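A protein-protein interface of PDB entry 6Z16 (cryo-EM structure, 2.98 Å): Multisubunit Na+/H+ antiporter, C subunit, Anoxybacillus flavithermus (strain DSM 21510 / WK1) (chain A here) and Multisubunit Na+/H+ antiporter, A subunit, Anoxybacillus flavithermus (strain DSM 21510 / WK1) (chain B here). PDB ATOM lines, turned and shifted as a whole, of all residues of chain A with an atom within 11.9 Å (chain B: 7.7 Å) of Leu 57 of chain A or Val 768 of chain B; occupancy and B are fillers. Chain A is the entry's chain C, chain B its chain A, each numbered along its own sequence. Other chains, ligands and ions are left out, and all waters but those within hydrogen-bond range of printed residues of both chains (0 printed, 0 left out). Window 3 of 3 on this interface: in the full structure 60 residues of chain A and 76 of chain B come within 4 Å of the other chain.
The side-chain carboxylate of Asp 66 of chain A sits at hydrogen-bond distance from the side-chain hydroxyl of Ser 764 of chain B (2.6 Å).
O of Lys 778 of chain B lies within hydrogen-bond range of N of Leu 57 of chain A (2.8 Å).
The backbone carbonyl oxygen of Pro 55 of chain A lies within hydrogen-bond range of the backbone NH of Met 780 of chain B, 3.3 Å away.
Pro 55 of chain A touches Asn 779 of chain B (O to OD1, 3.5 Å).
O of Lys 778 of chain B touches CA of Leu 56 of chain A, 3.7 Å away.
Leu 56 of chain A touches Asn 779 of chain B.
Leu 56 of chain A touches Met 780 of chain B (N to CE, 3.8 Å).
CD2 of Leu 57 of chain A touches O of Val 768 of chain B, at 3.9 Å.
Leu 57 of chain A touches Thr 771 of chain B.
Pro 67 of chain A touches Ser 764 of chain B.
Leu 68 of chain A touches Ser 764 of chain B (CD1 to OG, 3.8 Å).
CG of Leu 68 of chain A touches CE2 of Tyr 767 of chain B, 3.6 Å away.
Printed residues of chain B within 4 Å of Leu 56 of chain A: Lys 778, Asn 779 and Met 780.
Of chain B, only Val 768 (3.9 Å), Thr 771 (3.7 Å) and Lys 778 (2.8 Å) come within 4 Å of Leu 57 of chain A.
No residue of chain B comes within 4 Å of Gly 58 of chain A.
Printed residues of chain B within 4 Å of Asp 66 of chain A: Ser 764.
Ser 764 of chain B touches just these residues of chain A: Asp 66 (2.6 Å), Pro 67 (3.7 Å) and Leu 68 (3.8 Å).
No residue of chain A comes within 4 Å of Gln 765 of chain B.
No residue of chain A comes within 4 Å of Asp 769 of chain B.
No residue of chain A comes within 4 Å of Asn 770 of chain B.
Gly 777 of chain B touches none of the printed residues of chain A.
The nearest printed residue of chain B that does not touch Leu 57 of chain A is Met 780 of chain B (4.04 Å).
Hydrophobic or aromatic side chains of chain B within 4 Å of the printed part of chain A: Tyr 767 and Met 780.
Along chain B the printed residues that touch a printed residue of chain A span positions 764 to 780.
Printed residues of chain A that touch a printed residue of chain B: Pro 55, Leu 56, Leu 57, Asp 66, Pro 67 and Leu 68.
Along chain A the printed residues that touch a printed residue of chain B span positions 55 to 68.
Among the printed residues, 12 pairs touch across the chains.
Among the printed residues, no Asp or Glu carboxylate lies within 4 Å of a Lys or Arg side-chain nitrogen of the other chain.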
ATOM      1  N   LYS A  50      21.732  34.278  37.660  1.00  0.00           N
ATOM      2  CA  LYS A  50      23.035  34.211  38.309  1.00  0.00           C
ATOM      3  C   LYS A  50      24.124  34.675  37.346  1.00  0.00           C
ATOM      4  O   LYS A  50      24.051  34.428  36.142  1.00  0.00           O
ATOM      5  CB  LYS A  50      23.299  32.785  38.796  1.00  0.00           C
ATOM      6  CG  LYS A  50      24.579  32.589  39.597  1.00  0.00           C
ATOM      7  CD  LYS A  50      24.571  33.396  40.884  1.00  0.00           C
ATOM      8  CE  LYS A  50      23.550  32.859  41.871  1.00  0.00           C
ATOM      9  NZ  LYS A  50      23.945  31.535  42.420  1.00  0.00           N
ATOM     10  N   GLY A  52      27.199  35.456  35.029  1.00  0.00           N
ATOM     11  CA  GLY A  52      28.193  34.832  34.190  1.00  0.00           C
ATOM     12  C   GLY A  52      28.385  35.654  32.934  1.00  0.00           C
ATOM     13  O   GLY A  52      27.868  36.765  32.815  1.00  0.00           O
ATOM     14  N   ALA A  53      29.124  35.088  31.991  1.00  0.00           N
ATOM     15  CA  ALA A  53      29.424  35.775  30.747  1.00  0.00           C
ATOM     16  C   ALA A  53      28.208  35.798  29.826  1.00  0.00           C
ATOM     17  O   ALA A  53      27.299  34.982  29.975  1.00  0.00           O
ATOM     18  CB  ALA A  53      30.589  35.089  30.048  1.00  0.00           C
ATOM     19  N   PRO A  54      28.160  36.740  28.882  1.00  0.00           N
ATOM     20  CA  PRO A  54      27.159  36.661  27.824  1.00  0.00           C
ATOM     21  C   PRO A  54      27.359  35.411  26.990  1.00  0.00           C
ATOM     22  O   PRO A  54      28.481  34.878  26.903  1.00  0.00           O
ATOM     23  CB  PRO A  54      27.416  37.933  27.005  1.00  0.00           C
ATOM     24  CG  PRO A  54      27.976  38.870  27.970  1.00  0.00           C
ATOM     25  CD  PRO A  54      28.825  38.055  28.890  1.00  0.00           C
ATOM     26  N   PRO A  55      26.285  34.887  26.373  1.00  0.00           N
ATOM     27  CA  PRO A  55      26.391  33.582  25.707  1.00  0.00           C
ATOM     28  C   PRO A  55      27.195  33.624  24.416  1.00  0.00           C
ATOM     29  O   PRO A  55      26.639  33.612  23.316  1.00  0.00           O
ATOM     30  CB  PRO A  55      24.929  33.210  25.446  1.00  0.00           C
ATOM     31  CG  PRO A  55      24.230  34.500  25.371  1.00  0.00           C
ATOM     32  CD  PRO A  55      24.908  35.408  26.333  1.00  0.00           C
ATOM     33  N   LEU A  56      28.520  33.683  24.553  1.00  0.00           N
ATOM     34  CA  LEU A  56      29.433  33.821  23.425  1.00  0.00           C
ATOM     35  C   LEU A  56      30.682  33.027  23.759  1.00  0.00           C
ATOM     36  O   LEU A  56      31.333  33.310  24.766  1.00  0.00           O
ATOM     37  CB  LEU A  56      29.789  35.288  23.180  1.00  0.00           C
ATOM     38  CG  LEU A  56      28.708  36.299  22.796  1.00  0.00           C
ATOM     39  CD1 LEU A  56      29.272  37.697  22.809  1.00  0.00           C
ATOM     40  CD2 LEU A  56      28.126  35.978  21.448  1.00  0.00           C
ATOM     41  N   LEU A  57      31.023  32.044  22.931  1.00  0.00           N
ATOM     42  CA  LEU A  57      32.150  31.179  23.251  1.00  0.00           C
ATOM     43  C   LEU A  57      33.503  31.807  22.955  1.00  0.00           C
ATOM     44  O   LEU A  57      34.527  31.182  23.253  1.00  0.00           O
ATOM     45  CB  LEU A  57      32.044  29.852  22.504  1.00  0.00           C
ATOM     46  CG  LEU A  57      30.949  28.888  22.939  1.00  0.00           C
ATOM     47  CD1 LEU A  57      30.974  27.692  22.034  1.00  0.00           C
ATOM     48  CD2 LEU A  57      31.155  28.462  24.370  1.00  0.00           C
ATOM     49  N   GLY A  58      33.541  33.001  22.364  1.00  0.00           N
ATOM     50  CA  GLY A  58      34.800  33.717  22.261  1.00  0.00           C
ATOM     51  C   GLY A  58      35.315  34.146  23.620  1.00  0.00           C
ATOM     52  O   GLY A  58      36.498  33.993  23.931  1.00  0.00           O
ATOM     53  N   GLU A  59      34.427  34.684  24.449  1.00  0.00           N
ATOM     54  CA  GLU A  59      34.734  34.925  25.851  1.00  0.00           C
ATOM     55  C   GLU A  59      34.866  33.590  26.567  1.00  0.00           C
ATOM     56  O   GLU A  59      33.919  32.800  26.595  1.00  0.00           O
ATOM     57  CB  GLU A  59      33.633  35.772  26.478  1.00  0.00           C
ATOM     58  CG  GLU A  59      33.562  37.173  25.917  1.00  0.00           C
ATOM     59  CD  GLU A  59      32.392  37.955  26.462  1.00  0.00           C
ATOM     60  OE1 GLU A  59      31.545  37.339  27.140  1.00  0.00           O
ATOM     61  OE2 GLU A  59      32.320  39.177  26.221  1.00  0.00           O
ATOM     62  N   LYS A  60      36.029  33.341  27.159  1.00  0.00           N
ATOM     63  CA  LYS A  60      36.398  32.008  27.630  1.00  0.00           C
ATOM     64  C   LYS A  60      36.116  31.819  29.112  1.00  0.00           C
ATOM     65  O   LYS A  60      36.906  31.193  29.824  1.00  0.00           O
ATOM     66  CB  LYS A  60      37.866  31.731  27.333  1.00  0.00           C
ATOM     67  CG  LYS A  60      38.203  31.625  25.864  1.00  0.00           C
ATOM     68  CD  LYS A  60      39.666  31.274  25.692  1.00  0.00           C
ATOM     69  CE  LYS A  60      40.044  31.154  24.233  1.00  0.00           C
ATOM     70  NZ  LYS A  60      41.483  30.801  24.085  1.00  0.00           N
ATOM     71  N   ALA A  61      35.006  32.368  29.601  1.00  0.00           N
ATOM     72  CA  ALA A  61      34.694  32.337  31.019  1.00  0.00           C
ATOM     73  C   ALA A  61      34.332  30.930  31.479  1.00  0.00           C
ATOM     74  O   ALA A  61      34.032  30.042  30.679  1.00  0.00           O
ATOM     75  CB  ALA A  61      33.547  33.291  31.335  1.00  0.00           C
ATOM     76  N   SER A  62      34.370  30.740  32.800  1.00  0.00           N
ATOM     77  CA  SER A  62      34.148  29.417  33.372  1.00  0.00           C
ATOM     78  C   SER A  62      32.684  29.008  33.290  1.00  0.00           C
ATOM     79  O   SER A  62      32.377  27.842  33.028  1.00  0.00           O
ATOM     80  CB  SER A  62      34.633  29.387  34.819  1.00  0.00           C
ATOM     81  OG  SER A  62      34.396  28.122  35.407  1.00  0.00           O
ATOM     82  N   ARG A  63      31.768  29.947  33.512  1.00  0.00           N
ATOM     83  CA  ARG A  63      30.347  29.653  33.423  1.00  0.00           C
ATOM     84  C   ARG A  63      29.641  30.758  32.656  1.00  0.00           C
ATOM     85  O   ARG A  63      30.047  31.921  32.686  1.00  0.00           O
ATOM     86  CB  ARG A  63      29.714  29.472  34.808  1.00  0.00           C
ATOM     87  CG  ARG A  63      29.797  30.684  35.703  1.00  0.00           C
ATOM     88  CD  ARG A  63      29.138  30.422  37.037  1.00  0.00           C
ATOM     89  NE  ARG A  63      27.699  30.231  36.896  1.00  0.00           N
ATOM     90  CZ  ARG A  63      26.913  29.749  37.852  1.00  0.00           C
ATOM     91  NH1 ARG A  63      25.614  29.609  37.634  1.00  0.00           N
ATOM     92  NH2 ARG A  63      27.425  29.413  39.026  1.00  0.00           N
ATOM     93  N   TYR A  64      28.576  30.373  31.964  1.00  0.00           N
ATOM     94  CA  TYR A  64      27.830  31.253  31.083  1.00  0.00           C
ATOM     95  C   TYR A  64      26.400  31.405  31.580  1.00  0.00           C
ATOM     96  O   TYR A  64      25.889  30.573  32.328  1.00  0.00           O
ATOM     97  CB  TYR A  64      27.812  30.707  29.652  1.00  0.00           C
ATOM     98  CG  TYR A  64      29.153  30.693  28.965  1.00  0.00           C
ATOM     99  CD1 TYR A  64      29.621  31.808  28.284  1.00  0.00           C
ATOM    100  CD2 TYR A  64      29.955  29.563  29.005  1.00  0.00           C
ATOM    101  CE1 TYR A  64      30.843  31.793  27.657  1.00  0.00           C
ATOM    102  CE2 TYR A  64      31.178  29.541  28.385  1.00  0.00           C
ATOM    103  CZ  TYR A  64      31.617  30.657  27.715  1.00  0.00           C
ATOM    104  OH  TYR A  64      32.839  30.627  27.098  1.00  0.00           O
ATOM    105  N   VAL A  65      25.761  32.490  31.148  1.00  0.00           N
ATOM    106  CA  VAL A  65      24.324  32.643  31.315  1.00  0.00           C
ATOM    107  C   VAL A  65      23.617  31.632  30.413  1.00  0.00           C
ATOM    108  O   VAL A  65      24.137  31.249  29.358  1.00  0.00           O
ATOM    109  CB  VAL A  65      23.945  34.107  31.004  1.00  0.00           C
ATOM    110  CG1 VAL A  65      22.450  34.384  31.089  1.00  0.00           C
ATOM    111  CG2 VAL A  65      24.662  35.024  31.963  1.00  0.00           C
ATOM    112  N   ASP A  66      22.453  31.149  30.866  1.00  0.00           N
ATOM    113  CA  ASP A  66      21.670  30.129  30.171  1.00  0.00           C
ATOM    114  C   ASP A  66      21.274  30.584  28.765  1.00  0.00           C
ATOM    115  O   ASP A  66      20.680  31.661  28.612  1.00  0.00           O
ATOM    116  CB  ASP A  66      20.426  29.824  31.006  1.00  0.00           C
ATOM    117  CG  ASP A  66      19.702  28.560  30.582  1.00  0.00           C
ATOM    118  OD1 ASP A  66      20.128  27.879  29.635  1.00  0.00           O
ATOM    119  OD2 ASP A  66      18.668  28.252  31.205  1.00  0.00           O
ATOM    120  N   PRO A  67      21.599  29.808  27.717  1.00  0.00           N
ATOM    121  CA  PRO A  67      21.298  30.238  26.344  1.00  0.00           C
ATOM    122  C   PRO A  67      19.865  29.999  25.881  1.00  0.00           C
ATOM    123  O   PRO A  67      19.394  30.719  24.998  1.00  0.00           O
ATOM    124  CB  PRO A  67      22.269  29.403  25.506  1.00  0.00           C
ATOM    125  CG  PRO A  67      23.314  28.959  26.442  1.00  0.00           C
ATOM    126  CD  PRO A  67      22.630  28.759  27.735  1.00  0.00           C
ATOM    127  N   LEU A  68      19.187  28.980  26.427  1.00  0.00           N
ATOM    128  CA  LEU A  68      17.823  28.660  25.994  1.00  0.00           C
ATOM    129  C   LEU A  68      16.781  29.756  26.212  1.00  0.00           C
ATOM    130  O   LEU A  68      16.047  30.050  25.248  1.00  0.00           O
ATOM    131  CB  LEU A  68      17.343  27.352  26.631  1.00  0.00           C
ATOM    132  CG  LEU A  68      17.696  26.033  25.988  1.00  0.00           C
ATOM    133  CD1 LEU A  68      17.266  24.908  26.890  1.00  0.00           C
ATOM    134  CD2 LEU A  68      16.944  25.971  24.686  1.00  0.00           C
ATOM    135  N   PRO A  69      16.616  30.364  27.412  1.00  0.00           N
ATOM    136  CA  PRO A  69      15.510  31.318  27.570  1.00  0.00           C
ATOM    137  C   PRO A  69      15.657  32.549  26.714  1.00  0.00           C
ATOM    138  O   PRO A  69      14.643  33.113  26.313  1.00  0.00           O
ATOM    139  CB  PRO A  69      15.556  31.673  29.060  1.00  0.00           C
ATOM    140  CG  PRO A  69      16.283  30.597  29.686  1.00  0.00           C
ATOM    141  CD  PRO A  69      17.313  30.228  28.706  1.00  0.00           C
ATOM    142  N   GLN A  70      16.880  32.923  26.355  1.00  0.00           N
ATOM    143  CA  GLN A  70      17.080  34.075  25.487  1.00  0.00           C
ATOM    144  C   GLN A  70      16.573  33.801  24.074  1.00  0.00           C
ATOM    145  O   GLN A  70      15.913  34.655  23.467  1.00  0.00           O
ATOM    146  CB  GLN A  70      18.557  34.446  25.483  1.00  0.00           C
ATOM    147  CG  GLN A  70      19.071  34.849  26.841  1.00  0.00           C
ATOM    148  CD  GLN A  70      20.488  35.346  26.793  1.00  0.00           C
ATOM    149  OE1 GLN A  70      21.089  35.422  25.730  1.00  0.00           O
ATOM    150  NE2 GLN A  70      21.039  35.677  27.948  1.00  0.00           N
ATOM    151  N   ILE B 763      19.451  21.684  30.715  1.00  0.00           N
ATOM    152  CA  ILE B 763      20.074  20.931  29.629  1.00  0.00           C
ATOM    153  C   ILE B 763      20.928  21.829  28.744  1.00  0.00           C
ATOM    154  O   ILE B 763      21.103  21.551  27.554  1.00  0.00           O
ATOM    155  CB  ILE B 763      19.017  20.213  28.773  1.00  0.00           C
ATOM    156  CG1 ILE B 763      17.957  21.212  28.293  1.00  0.00           C
ATOM    157  CG2 ILE B 763      18.439  19.041  29.519  1.00  0.00           C
ATOM    158  CD1 ILE B 763      17.088  20.702  27.180  1.00  0.00           C
ATOM    159  N   SER B 764      21.476  22.901  29.300  1.00  0.00           N
ATOM    160  CA  SER B 764      22.262  23.829  28.504  1.00  0.00           C
ATOM    161  C   SER B 764      23.760  23.608  28.616  1.00  0.00           C
ATOM    162  O   SER B 764      24.523  24.365  28.016  1.00  0.00           O
ATOM    163  CB  SER B 764      21.924  25.263  28.888  1.00  0.00           C
ATOM    164  OG  SER B 764      20.595  25.566  28.511  1.00  0.00           O
ATOM    165  N   GLN B 765      24.204  22.604  29.370  1.00  0.00           N
ATOM    166  CA  GLN B 765      25.612  22.231  29.335  1.00  0.00           C
ATOM    167  C   GLN B 765      25.978  21.627  27.986  1.00  0.00           C
ATOM    168  O   GLN B 765      27.101  21.807  27.502  1.00  0.00           O
ATOM    169  CB  GLN B 765      25.910  21.254  30.470  1.00  0.00           C
ATOM    170  CG  GLN B 765      27.363  20.860  30.637  1.00  0.00           C
ATOM    171  CD  GLN B 765      28.251  22.017  31.040  1.00  0.00           C
ATOM    172  OE1 GLN B 765      29.032  22.520  30.238  1.00  0.00           O
ATOM    173  NE2 GLN B 765      28.141  22.439  32.293  1.00  0.00           N
ATOM    174  N   TYR B 766      25.023  20.942  27.355  1.00  0.00           N
ATOM    175  CA  TYR B 766      25.212  20.399  26.016  1.00  0.00           C
ATOM    176  C   TYR B 766      25.393  21.510  24.989  1.00  0.00           C
ATOM    177  O   TYR B 766      26.218  21.393  24.078  1.00  0.00           O
ATOM    178  CB  TYR B 766      24.006  19.535  25.657  1.00  0.00           C
ATOM    179  CG  TYR B 766      24.102  18.747  24.373  1.00  0.00           C
ATOM    180  CD1 TYR B 766      24.766  17.531  24.334  1.00  0.00           C
ATOM    181  CD2 TYR B 766      23.515  19.213  23.207  1.00  0.00           C
ATOM    182  CE1 TYR B 766      24.845  16.805  23.169  1.00  0.00           C
ATOM    183  CE2 TYR B 766      23.597  18.498  22.036  1.00  0.00           C
ATOM    184  CZ  TYR B 766      24.260  17.294  22.024  1.00  0.00           C
ATOM    185  OH  TYR B 766      24.349  16.562  20.869  1.00  0.00           O
ATOM    186  N   TYR B 767      24.645  22.602  25.132  1.00  0.00           N
ATOM    187  CA  TYR B 767      24.707  23.676  24.151  1.00  0.00           C
ATOM    188  C   TYR B 767      25.958  24.521  24.307  1.00  0.00           C
ATOM    189  O   TYR B 767      26.447  25.071  23.321  1.00  0.00           O
ATOM    190  CB  TYR B 767      23.482  24.570  24.270  1.00  0.00           C
ATOM    191  CG  TYR B 767      22.183  23.895  23.930  1.00  0.00           C
ATOM    192  CD1 TYR B 767      22.144  22.758  23.139  1.00  0.00           C
ATOM    193  CD2 TYR B 767      20.994  24.375  24.441  1.00  0.00           C
ATOM    194  CE1 TYR B 767      20.952  22.144  22.844  1.00  0.00           C
ATOM    195  CE2 TYR B 767      19.804  23.774  24.146  1.00  0.00           C
ATOM    196  CZ  TYR B 767      19.785  22.660  23.354  1.00  0.00           C
ATOM    197  OH  TYR B 767      18.587  22.067  23.075  1.00  0.00           O
ATOM    198  N   VAL B 768      26.477  24.661  25.529  1.00  0.00           N
ATOM    199  CA  VAL B 768      27.751  25.348  25.711  1.00  0.00           C
ATOM    200  C   VAL B 768      28.926  24.418  25.489  1.00  0.00           C
ATOM    201  O   VAL B 768      30.070  24.879  25.436  1.00  0.00           O
ATOM    202  CB  VAL B 768      27.886  25.977  27.110  1.00  0.00           C
ATOM    203  CG1 VAL B 768      26.704  26.874  27.421  1.00  0.00           C
ATOM    204  CG2 VAL B 768      28.053  24.920  28.173  1.00  0.00           C
ATOM    205  N   ASP B 769      28.678  23.117  25.376  1.00  0.00           N
ATOM    206  CA  ASP B 769      29.733  22.155  25.121  1.00  0.00           C
ATOM    207  C   ASP B 769      29.821  21.772  23.652  1.00  0.00           C
ATOM    208  O   ASP B 769      30.842  21.222  23.228  1.00  0.00           O
ATOM    209  CB  ASP B 769      29.485  20.901  25.966  1.00  0.00           C
ATOM    210  CG  ASP B 769      30.731  20.073  26.188  1.00  0.00           C
ATOM    211  OD1 ASP B 769      31.829  20.483  25.761  1.00  0.00           O
ATOM    212  OD2 ASP B 769      30.606  18.994  26.802  1.00  0.00           O
ATOM    213  N   ASN B 770      28.784  22.058  22.861  1.00  0.00           N
ATOM    214  CA  ASN B 770      28.746  21.575  21.487  1.00  0.00           C
ATOM    215  C   ASN B 770      28.266  22.635  20.505  1.00  0.00           C
ATOM    216  O   ASN B 770      27.706  22.298  19.459  1.00  0.00           O
ATOM    217  CB  ASN B 770      27.859  20.337  21.373  1.00  0.00           C
ATOM    218  CG  ASN B 770      28.485  19.115  22.005  1.00  0.00           C
ATOM    219  OD1 ASN B 770      29.671  18.850  21.827  1.00  0.00           O
ATOM    220  ND2 ASN B 770      27.695  18.367  22.758  1.00  0.00           N
ATOM    221  N   THR B 771      28.465  23.916  20.809  1.00  0.00           N
ATOM    222  CA  THR B 771      28.142  24.934  19.818  1.00  0.00           C
ATOM    223  C   THR B 771      29.247  25.033  18.777  1.00  0.00           C
ATOM    224  O   THR B 771      28.975  25.223  17.587  1.00  0.00           O
ATOM    225  CB  THR B 771      27.895  26.283  20.498  1.00  0.00           C
ATOM    226  OG1 THR B 771      26.794  26.161  21.398  1.00  0.00           O
ATOM    227  CG2 THR B 771      27.549  27.365  19.498  1.00  0.00           C
ATOM    228  N   TYR B 772      30.495  24.856  19.192  1.00  0.00           N
ATOM    229  CA  TYR B 772      31.606  24.908  18.255  1.00  0.00           C
ATOM    230  C   TYR B 772      32.150  23.536  17.885  1.00  0.00           C
ATOM    231  O   TYR B 772      32.605  23.353  16.753  1.00  0.00           O
ATOM    232  CB  TYR B 772      32.735  25.773  18.824  1.00  0.00           C
ATOM    233  CG  TYR B 772      33.926  25.884  17.912  1.00  0.00           C
ATOM    234  CD1 TYR B 772      33.867  26.649  16.756  1.00  0.00           C
ATOM    235  CD2 TYR B 772      35.109  25.220  18.205  1.00  0.00           C
ATOM    236  CE1 TYR B 772      34.950  26.745  15.917  1.00  0.00           C
ATOM    237  CE2 TYR B 772      36.198  25.310  17.373  1.00  0.00           C
ATOM    238  CZ  TYR B 772      36.116  26.075  16.233  1.00  0.00           C
ATOM    239  OH  TYR B 772      37.207  26.165  15.403  1.00  0.00           O
ATOM    240  N   GLU B 773      32.112  22.562  18.795  1.00  0.00           N
ATOM    241  CA  GLU B 773      32.636  21.240  18.475  1.00  0.00           C
ATOM    242  C   GLU B 773      31.759  20.478  17.489  1.00  0.00           C
ATOM    243  O   GLU B 773      32.266  19.597  16.789  1.00  0.00           O
ATOM    244  CB  GLU B 773      32.803  20.412  19.748  1.00  0.00           C
ATOM    245  CG  GLU B 773      33.877  20.919  20.696  1.00  0.00           C
ATOM    246  CD  GLU B 773      35.284  20.738  20.154  1.00  0.00           C
ATOM    247  OE1 GLU B 773      35.519  19.767  19.403  1.00  0.00           O
ATOM    248  OE2 GLU B 773      36.160  21.564  20.488  1.00  0.00           O
ATOM    249  N   GLY B 777      29.938  27.700  15.015  1.00  0.00           N
ATOM    250  CA  GLY B 777      29.517  28.945  15.622  1.00  0.00           C
ATOM    251  C   GLY B 777      30.177  29.160  16.961  1.00  0.00           C
ATOM    252  O   GLY B 777      30.607  28.213  17.629  1.00  0.00           O
ATOM    253  N   LYS B 778      30.269  30.432  17.332  1.00  0.00           N
ATOM    254  CA  LYS B 778      30.685  30.850  18.662  1.00  0.00           C
ATOM    255  C   LYS B 778      29.568  31.519  19.435  1.00  0.00           C
ATOM    256  O   LYS B 778      29.497  31.370  20.655  1.00  0.00           O
ATOM    257  CB  LYS B 778      31.877  31.806  18.573  1.00  0.00           C
ATOM    258  CG  LYS B 778      33.137  31.188  18.016  1.00  0.00           C
ATOM    259  CD  LYS B 778      33.735  30.193  18.974  1.00  0.00           C
ATOM    260  CE  LYS B 778      35.030  29.648  18.429  1.00  0.00           C
ATOM    261  NZ  LYS B 778      36.070  30.706  18.353  1.00  0.00           N
ATOM    262  N   ASN B 779      28.714  32.269  18.744  1.00  0.00           N
ATOM    263  CA  ASN B 779      27.466  32.744  19.318  1.00  0.00           C
ATOM    264  C   ASN B 779      26.604  31.548  19.687  1.00  0.00           C
ATOM    265  O   ASN B 779      26.638  30.515  19.025  1.00  0.00           O
ATOM    266  CB  ASN B 779      26.734  33.620  18.308  1.00  0.00           C
ATOM    267  CG  ASN B 779      25.630  34.431  18.926  1.00  0.00           C
ATOM    268  OD1 ASN B 779      25.381  34.355  20.123  1.00  0.00           O
ATOM    269  ND2 ASN B 779      24.970  35.234  18.112  1.00  0.00           N
ATOM    270  N   MET B 780      25.843  31.668  20.769  1.00  0.00           N
ATOM    271  CA  MET B 780      24.997  30.555  21.168  1.00  0.00           C
ATOM    272  C   MET B 780      23.514  30.824  21.051  1.00  0.00           C
ATOM    273  O   MET B 780      22.757  29.870  20.919  1.00  0.00           O
ATOM    274  CB  MET B 780      25.315  30.111  22.597  1.00  0.00           C
ATOM    275  CG  MET B 780      26.604  29.353  22.668  1.00  0.00           C
ATOM    276  SD  MET B 780      26.944  28.666  24.283  1.00  0.00           S
ATOM    277  CE  MET B 780      27.545  30.095  25.155  1.00  0.00           C
ATOM    278  N   ILE B 784      21.402  28.231  18.474  1.00  0.00           N
ATOM    279  CA  ILE B 784      20.124  27.656  18.899  1.00  0.00           C
ATOM    280  C   ILE B 784      19.009  28.062  17.942  1.00  0.00           C
ATOM    281  O   ILE B 784      18.157  27.244  17.585  1.00  0.00           O
ATOM    282  CB  ILE B 784      19.804  28.057  20.355  1.00  0.00           C
ATOM    283  CG1 ILE B 784      20.795  27.427  21.325  1.00  0.00           C
ATOM    284  CG2 ILE B 784      18.411  27.633  20.765  1.00  0.00           C
ATOM    285  CD1 ILE B 784      20.805  25.961  21.282  1.00  0.00           C
ATOM    286  N   PHE B 788      20.356  24.161  16.252  1.00  0.00           N
ATOM    287  CA  PHE B 788      19.838  23.161  17.185  1.00  0.00           C
ATOM    288  C   PHE B 788      18.317  23.146  17.191  1.00  0.00           C
ATOM    289  O   PHE B 788      17.697  22.082  17.103  1.00  0.00           O
ATOM    290  CB  PHE B 788      20.355  23.409  18.598  1.00  0.00           C
ATOM    291  CG  PHE B 788      21.784  23.045  18.803  1.00  0.00           C
ATOM    292  CD1 PHE B 788      22.153  21.724  18.931  1.00  0.00           C
ATOM    293  CD2 PHE B 788      22.748  24.021  18.940  1.00  0.00           C
ATOM    294  CE1 PHE B 788      23.463  21.381  19.145  1.00  0.00           C
ATOM    295  CE2 PHE B 788      24.062  23.679  19.163  1.00  0.00           C
ATOM    296  CZ  PHE B 788      24.417  22.359  19.265  1.00  0.00           C
